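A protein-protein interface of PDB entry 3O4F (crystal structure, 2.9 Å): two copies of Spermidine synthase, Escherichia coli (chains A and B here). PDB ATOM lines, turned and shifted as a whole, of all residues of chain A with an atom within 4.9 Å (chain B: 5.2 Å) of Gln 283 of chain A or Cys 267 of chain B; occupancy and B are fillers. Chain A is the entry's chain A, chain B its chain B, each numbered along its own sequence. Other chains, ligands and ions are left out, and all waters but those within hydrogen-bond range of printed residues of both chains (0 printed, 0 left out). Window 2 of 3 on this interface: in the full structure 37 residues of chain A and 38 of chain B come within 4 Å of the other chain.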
ATOM      1  N   LEU A 281      -9.996  22.911 -16.943  1.00  0.00           N
ATOM      2  CA  LEU A 281     -11.046  23.882 -16.998  1.00  0.00           C
ATOM      3  C   LEU A 281     -11.641  24.083 -15.618  1.00  0.00           C
ATOM      4  O   LEU A 281     -11.799  23.127 -14.829  1.00  0.00           O
ATOM      5  CB  LEU A 281     -12.128  23.412 -17.986  1.00  0.00           C
ATOM      6  CG  LEU A 281     -11.718  23.205 -19.459  1.00  0.00           C
ATOM      7  CD1 LEU A 281     -12.897  23.018 -20.364  1.00  0.00           C
ATOM      8  CD2 LEU A 281     -10.914  24.339 -19.978  1.00  0.00           C
ATOM      9  N   PRO A 282     -12.007  25.313 -15.327  1.00  0.00           N
ATOM     10  CA  PRO A 282     -12.645  25.571 -14.080  1.00  0.00           C
ATOM     11  C   PRO A 282     -13.940  24.812 -13.934  1.00  0.00           C
ATOM     12  O   PRO A 282     -14.584  24.471 -14.901  1.00  0.00           O
ATOM     13  CB  PRO A 282     -12.886  27.072 -14.092  1.00  0.00           C
ATOM     14  CG  PRO A 282     -12.721  27.510 -15.443  1.00  0.00           C
ATOM     15  CD  PRO A 282     -11.947  26.494 -16.182  1.00  0.00           C
ATOM     16  N   GLN A 283     -14.286  24.568 -12.679  1.00  0.00           N
ATOM     17  CA  GLN A 283     -15.324  23.639 -12.346  1.00  0.00           C
ATOM     18  C   GLN A 283     -16.647  24.027 -12.979  1.00  0.00           C
ATOM     19  O   GLN A 283     -17.327  23.166 -13.559  1.00  0.00           O
ATOM     20  CB  GLN A 283     -15.466  23.535 -10.844  1.00  0.00           C
ATOM     21  CG  GLN A 283     -16.259  22.332 -10.400  1.00  0.00           C
ATOM     22  CD  GLN A 283     -15.879  21.044 -11.138  1.00  0.00           C
ATOM     23  OE1 GLN A 283     -14.688  20.714 -11.301  1.00  0.00           O
ATOM     24  NE2 GLN A 283     -16.893  20.324 -11.593  1.00  0.00           N
ATOM     25  N   TYR A 284     -17.000  25.313 -12.910  1.00  0.00           N
ATOM     26  CA  TYR A 284     -18.291  25.760 -13.457  1.00  0.00           C
ATOM     27  C   TYR A 284     -18.365  25.386 -14.924  1.00  0.00           C
ATOM     28  O   TYR A 284     -19.376  24.944 -15.414  1.00  0.00           O
ATOM     29  CB  TYR A 284     -18.534  27.251 -13.239  1.00  0.00           C
ATOM     30  CG  TYR A 284     -17.682  28.163 -14.036  1.00  0.00           C
ATOM     31  CD1 TYR A 284     -16.545  28.709 -13.511  1.00  0.00           C
ATOM     32  CD2 TYR A 284     -18.026  28.493 -15.306  1.00  0.00           C
ATOM     33  CE1 TYR A 284     -15.736  29.542 -14.258  1.00  0.00           C
ATOM     34  CE2 TYR A 284     -17.248  29.343 -16.054  1.00  0.00           C
ATOM     35  CZ  TYR A 284     -16.099  29.842 -15.531  1.00  0.00           C
ATOM     36  OH  TYR A 284     -15.323  30.685 -16.260  1.00  0.00           O
ATOM     37  N   LEU A 285     -17.272  25.501 -15.629  1.00  0.00           N
ATOM     38  CA  LEU A 285     -17.340  25.209 -17.053  1.00  0.00           C
ATOM     39  C   LEU A 285     -17.601  23.730 -17.297  1.00  0.00           C
ATOM     40  O   LEU A 285     -18.287  23.355 -18.248  1.00  0.00           O
ATOM     41  CB  LEU A 285     -16.060  25.642 -17.761  1.00  0.00           C
ATOM     42  CG  LEU A 285     -16.132  25.500 -19.266  1.00  0.00           C
ATOM     43  CD1 LEU A 285     -17.270  26.282 -19.893  1.00  0.00           C
ATOM     44  CD2 LEU A 285     -14.989  25.879 -19.931  1.00  0.00           C
ATOM     45  N   GLN A 286     -17.059  22.895 -16.434  1.00  0.00           N
ATOM     46  CA  GLN A 286     -17.181  21.477 -16.638  1.00  0.00           C
ATOM     47  C   GLN A 286     -18.582  21.079 -16.353  1.00  0.00           C
ATOM     48  O   GLN A 286     -19.171  20.286 -17.104  1.00  0.00           O
ATOM     49  CB  GLN A 286     -16.218  20.697 -15.767  1.00  0.00           C
ATOM     50  CG  GLN A 286     -14.788  20.926 -16.198  1.00  0.00           C
ATOM     51  CD  GLN A 286     -13.822  20.003 -15.584  1.00  0.00           C
ATOM     52  OE1 GLN A 286     -14.065  18.830 -15.482  1.00  0.00           O
ATOM     53  NE2 GLN A 286     -12.704  20.535 -15.127  1.00  0.00           N
ATOM     54  N   ASP A 287     -19.145  21.636 -15.288  1.00  0.00           N
ATOM     55  CA  ASP A 287     -20.510  21.264 -14.930  1.00  0.00           C
ATOM     56  C   ASP A 287     -21.504  21.747 -16.026  1.00  0.00           C
ATOM     57  O   ASP A 287     -22.520  21.093 -16.325  1.00  0.00           O
ATOM     58  CB  ASP A 287     -20.912  21.839 -13.556  1.00  0.00           C
ATOM     59  CG  ASP A 287     -19.933  21.490 -12.456  1.00  0.00           C
ATOM     60  OD1 ASP A 287     -19.410  20.358 -12.484  1.00  0.00           O
ATOM     61  OD2 ASP A 287     -19.686  22.357 -11.585  1.00  0.00           O
ATOM     62  N   GLU B  71     -11.615  30.685  -3.625  1.00  0.00           N
ATOM     63  CA  GLU B  71     -11.368  29.281  -3.728  1.00  0.00           C
ATOM     64  C   GLU B  71      -9.912  29.034  -4.013  1.00  0.00           C
ATOM     65  O   GLU B  71      -9.277  28.295  -3.354  1.00  0.00           O
ATOM     66  CB  GLU B  71     -12.222  28.687  -4.837  1.00  0.00           C
ATOM     67  CG  GLU B  71     -13.566  28.180  -4.401  1.00  0.00           C
ATOM     68  CD  GLU B  71     -14.390  27.638  -5.499  1.00  0.00           C
ATOM     69  OE1 GLU B  71     -13.843  27.238  -6.488  1.00  0.00           O
ATOM     70  OE2 GLU B  71     -15.595  27.593  -5.383  1.00  0.00           O
ATOM     71  N   HIS B  75      -7.957  26.804  -1.142  1.00  0.00           N
ATOM     72  CA  HIS B  75      -7.738  25.392  -1.280  1.00  0.00           C
ATOM     73  C   HIS B  75      -6.388  24.984  -1.773  1.00  0.00           C
ATOM     74  O   HIS B  75      -5.837  24.032  -1.329  1.00  0.00           O
ATOM     75  CB  HIS B  75      -8.834  24.768  -2.081  1.00  0.00           C
ATOM     76  CG  HIS B  75     -10.188  25.227  -1.687  1.00  0.00           C
ATOM     77  ND1 HIS B  75     -10.562  25.375  -0.380  1.00  0.00           N
ATOM     78  CD2 HIS B  75     -11.257  25.580  -2.421  1.00  0.00           C
ATOM     79  CE1 HIS B  75     -11.804  25.796  -0.322  1.00  0.00           C
ATOM     80  NE2 HIS B  75     -12.245  25.941  -1.550  1.00  0.00           N
ATOM     81  N   GLU B 100     -14.497  29.718   3.037  1.00  0.00           N
ATOM     82  CA  GLU B 100     -13.868  28.599   2.335  1.00  0.00           C
ATOM     83  C   GLU B 100     -13.023  27.790   3.310  1.00  0.00           C
ATOM     84  O   GLU B 100     -13.140  26.576   3.400  1.00  0.00           O
ATOM     85  CB  GLU B 100     -13.062  29.059   1.120  1.00  0.00           C
ATOM     86  CG  GLU B 100     -13.927  29.757   0.055  1.00  0.00           C
ATOM     87  CD  GLU B 100     -14.873  28.820  -0.741  1.00  0.00           C
ATOM     88  OE1 GLU B 100     -14.541  27.622  -0.970  1.00  0.00           O
ATOM     89  OE2 GLU B 100     -15.952  29.317  -1.159  1.00  0.00           O
ATOM     90  N   ARG B 103     -14.800  25.222   5.151  1.00  0.00           N
ATOM     91  CA  ARG B 103     -15.290  24.029   4.475  1.00  0.00           C
ATOM     92  C   ARG B 103     -14.406  22.807   4.615  1.00  0.00           C
ATOM     93  O   ARG B 103     -14.797  21.713   4.222  1.00  0.00           O
ATOM     94  CB  ARG B 103     -15.578  24.302   3.013  1.00  0.00           C
ATOM     95  CG  ARG B 103     -16.714  25.305   2.870  1.00  0.00           C
ATOM     96  CD  ARG B 103     -16.689  26.056   1.569  1.00  0.00           C
ATOM     97  NE  ARG B 103     -16.960  25.181   0.431  1.00  0.00           N
ATOM     98  CZ  ARG B 103     -17.744  25.501  -0.590  1.00  0.00           C
ATOM     99  NH1 ARG B 103     -17.915  24.612  -1.567  1.00  0.00           N
ATOM    100  NH2 ARG B 103     -18.375  26.685  -0.619  1.00  0.00           N
ATOM    101  N   PHE B 260      -8.769  15.779  -2.368  1.00  0.00           N
ATOM    102  CA  PHE B 260      -9.969  16.475  -2.728  1.00  0.00           C
ATOM    103  C   PHE B 260     -11.224  15.642  -2.525  1.00  0.00           C
ATOM    104  O   PHE B 260     -12.228  16.131  -2.086  1.00  0.00           O
ATOM    105  CB  PHE B 260      -9.861  16.986  -4.156  1.00  0.00           C
ATOM    106  CG  PHE B 260     -10.970  17.879  -4.560  1.00  0.00           C
ATOM    107  CD1 PHE B 260     -11.126  19.076  -3.982  1.00  0.00           C
ATOM    108  CD2 PHE B 260     -11.862  17.511  -5.502  1.00  0.00           C
ATOM    109  CE1 PHE B 260     -12.119  19.863  -4.334  1.00  0.00           C
ATOM    110  CE2 PHE B 260     -12.845  18.312  -5.830  1.00  0.00           C
ATOM    111  CZ  PHE B 260     -12.974  19.480  -5.246  1.00  0.00           C
ATOM    112  N   LEU B 265     -15.045  18.863  -0.849  1.00  0.00           N
ATOM    113  CA  LEU B 265     -15.566  20.127  -1.201  1.00  0.00           C
ATOM    114  C   LEU B 265     -16.274  19.954  -2.472  1.00  0.00           C
ATOM    115  O   LEU B 265     -16.022  19.033  -3.194  1.00  0.00           O
ATOM    116  CB  LEU B 265     -14.436  21.082  -1.455  1.00  0.00           C
ATOM    117  CG  LEU B 265     -13.437  21.370  -0.370  1.00  0.00           C
ATOM    118  CD1 LEU B 265     -12.121  21.311  -0.948  1.00  0.00           C
ATOM    119  CD2 LEU B 265     -13.660  22.709   0.106  1.00  0.00           C
ATOM    120  N   LYS B 266     -17.188  20.849  -2.751  1.00  0.00           N
ATOM    121  CA  LYS B 266     -17.733  20.942  -4.061  1.00  0.00           C
ATOM    122  C   LYS B 266     -17.450  22.371  -4.308  1.00  0.00           C
ATOM    123  O   LYS B 266     -18.093  23.206  -3.749  1.00  0.00           O
ATOM    124  CB  LYS B 266     -19.231  20.716  -4.036  1.00  0.00           C
ATOM    125  CG  LYS B 266     -19.845  20.291  -5.365  1.00  0.00           C
ATOM    126  CD  LYS B 266     -19.080  19.157  -6.012  1.00  0.00           C
ATOM    127  CE  LYS B 266     -18.897  19.372  -7.509  1.00  0.00           C
ATOM    128  NZ  LYS B 266     -19.753  20.437  -8.054  1.00  0.00           N
ATOM    129  N   CYS B 267     -16.477  22.645  -5.149  1.00  0.00           N
ATOM    130  CA  CYS B 267     -16.112  23.991  -5.501  1.00  0.00           C
ATOM    131  C   CYS B 267     -16.727  24.356  -6.805  1.00  0.00           C
ATOM    132  O   CYS B 267     -17.348  23.512  -7.450  1.00  0.00           O
ATOM    133  CB  CYS B 267     -14.608  24.113  -5.633  1.00  0.00           C
ATOM    134  SG  CYS B 267     -13.800  23.860  -4.099  1.00  0.00           S
ATOM    135  N   ARG B 268     -16.532  25.612  -7.196  1.00  0.00           N
ATOM    136  CA  ARG B 268     -17.085  26.135  -8.438  1.00  0.00           C
ATOM    137  C   ARG B 268     -16.067  26.651  -9.472  1.00  0.00           C
ATOM    138  O   ARG B 268     -16.407  26.909 -10.626  1.00  0.00           O
ATOM    139  CB  ARG B 268     -18.043  27.244  -8.088  1.00  0.00           C
ATOM    140  CG  ARG B 268     -19.343  26.708  -7.526  1.00  0.00           C
ATOM    141  CD  ARG B 268     -20.512  27.672  -7.798  1.00  0.00           C
ATOM    142  NE  ARG B 268     -20.512  28.703  -6.780  1.00  0.00           N
ATOM    143  CZ  ARG B 268     -20.424  30.013  -6.999  1.00  0.00           C
ATOM    144  NH1 ARG B 268     -20.362  30.532  -8.219  1.00  0.00           N
ATOM    145  NH2 ARG B 268     -20.390  30.815  -5.953  1.00  0.00           N
ATOM    146  N   TYR B 269     -14.831  26.818  -9.036  1.00  0.00           N
ATOM    147  CA  TYR B 269     -13.737  27.026  -9.929  1.00  0.00           C
ATOM    148  C   TYR B 269     -12.736  25.905  -9.687  1.00  0.00           C
ATOM    149  O   TYR B 269     -12.434  25.152 -10.617  1.00  0.00           O
ATOM    150  CB  TYR B 269     -13.120  28.383  -9.679  1.00  0.00           C
ATOM    151  CG  TYR B 269     -12.167  28.860 -10.791  1.00  0.00           C
ATOM    152  CD1 TYR B 269     -12.629  29.572 -11.878  1.00  0.00           C
ATOM    153  CD2 TYR B 269     -10.821  28.601 -10.718  1.00  0.00           C
ATOM    154  CE1 TYR B 269     -11.812  29.964 -12.851  1.00  0.00           C
ATOM    155  CE2 TYR B 269      -9.981  28.995 -11.690  1.00  0.00           C
ATOM    156  CZ  TYR B 269     -10.463  29.675 -12.779  1.00  0.00           C
ATOM    157  OH  TYR B 269      -9.550  30.101 -13.778  1.00  0.00           O
ATOM    158  N   TYR B 270     -12.271  25.765  -8.446  1.00  0.00           N
ATOM    159  CA  TYR B 270     -11.193  24.860  -8.112  1.00  0.00           C
ATOM    160  C   TYR B 270     -11.499  23.440  -8.447  1.00  0.00           C
ATOM    161  O   TYR B 270     -12.632  22.988  -8.278  1.00  0.00           O
ATOM    162  CB  TYR B 270     -10.936  24.897  -6.624  1.00  0.00           C
ATOM    163  CG  TYR B 270      -9.821  23.981  -6.135  1.00  0.00           C
ATOM    164  CD1 TYR B 270      -8.543  24.463  -5.982  1.00  0.00           C
ATOM    165  CD2 TYR B 270     -10.074  22.644  -5.790  1.00  0.00           C
ATOM    166  CE1 TYR B 270      -7.548  23.668  -5.514  1.00  0.00           C
ATOM    167  CE2 TYR B 270      -9.073  21.836  -5.330  1.00  0.00           C
ATOM    168  CZ  TYR B 270      -7.815  22.363  -5.179  1.00  0.00           C
ATOM    169  OH  TYR B 270      -6.799  21.584  -4.714  1.00  0.00           O
ATOM    170  N   ASN B 271     -10.458  22.725  -8.867  1.00  0.00           N
ATOM    171  CA  ASN B 271     -10.460  21.242  -8.919  1.00  0.00           C
ATOM    172  C   ASN B 271      -8.974  20.778  -9.035  1.00  0.00           C
ATOM    173  O   ASN B 271      -8.060  21.605  -9.245  1.00  0.00           O
ATOM    174  CB  ASN B 271     -11.308  20.760 -10.074  1.00  0.00           C
ATOM    175  CG  ASN B 271     -10.935  21.479 -11.370  1.00  0.00           C
ATOM    176  OD1 ASN B 271      -9.742  21.585 -11.722  1.00  0.00           O
ATOM    177  ND2 ASN B 271     -11.944  22.020 -12.066  1.00  0.00           N
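No position is printed for both chains.
Of the 11 pairs that touch across the chains among the printed residues, none has its exchanged pair printed and touching as well.
Of the printed residues of chain B, Leu 281 of chain A touches Asn 271.
Printed residues of chain B within 4 Å of Gln 286 of chain A: Asn 271 (3.5 Å).
Glu 100 of chain B touches none of the printed residues of chain A.
Of chain A, only Gln 283 (3.4 Å) comes within 4 Å of Cys 267 of chain B.
Of the printed residues of chain A, Tyr 269 of chain B touches Pro 282 (3.3 Å), Gln 283 (2.8 Å) and Tyr 284 (3.9 Å).
The nearest residue of chain B that does not touch Gln 283 of chain A is Lys 266 of chain B (4.6 Å).
The nearest printed residue of chain A that does not touch Cys 267 of chain B is Asp 287 of chain A (4.9 Å).
The nearest printed residue of chain A that does not touch Tyr 269 of chain B is Leu 281 of chain A (4.7 Å).
Pro 282 of chain A touches Tyr 269 of chain B.
Asn 271 of chain B touches Pro 282 of chain A (ND2 to C, 3.9 Å).
Cys 267 of chain B touches Gln 283 of chain A.
Arg 268 of chain B touches Gln 283 of chain A.
Tyr 270 of chain B touches Gln 283 of chain A (O to CB, 3.9 Å).
CE1 of Tyr 284 of chain A touches CD1 of Tyr 269 of chain B (3.9 Å).
The backbone NH of Gln 283 of chain A sits at hydrogen-bond distance from the backbone carbonyl oxygen of Tyr 269 of chain B, at 2.8 Å.
ND2 of Asn 271 of chain B sits close to NE2 of Gln 286 of chain A (3.5 Å).
The side-chain amide nitrogen of Asn 271 of chain B sits at hydrogen-bond distance from the side-chain amide oxygen of Gln 283 of chain A.
The backbone NH (N) of Tyr 284 of chain A is in hydrogen-bond range of the backbone carbonyl oxygen (O) of Arg 268 of chain B.
The backbone carbonyl oxygen (O) of Leu 281 of chain A sits at hydrogen-bond distance from the side-chain amide nitrogen (ND2) of Asn 271 of chain B.
The side-chain carboxylate (OE1) of Glu 71 of chain B sits at hydrogen-bond distance from the backbone NH (N) of Tyr 269 of chain B (2.8 Å).
OD1 of Asp 287 of chain A is in hydrogen-bond range of NE2 of Gln 283 of chain A.
The side-chain carboxylate (OE1) of Glu 71 of chain B lies within hydrogen-bond range of the backbone NH (N) of Tyr 270 of chain B, at 2.9 Å.
SG of Cys 267 of chain B lies close to NE2 of His 75 of chain B.
The backbone carbonyl oxygen of Tyr 269 of chain B lies within hydrogen-bond range of the side-chain amide nitrogen of Asn 271 of chain B (3.5 Å).
The backbone carbonyl oxygen of Leu 281 of chain A is in hydrogen-bond range of the side-chain amide nitrogen of Gln 286 of chain A.
Hydrophobic or aromatic side chains of chain A within 4 Å of the printed part of chain B: Pro 282 and Tyr 284.
Among the printed residues, 11 pairs touch across the chains.
Among the printed residues, no Asp or Glu carboxylate lies within 4 Å of a Lys or Arg side-chain nitrogen of the other chain.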
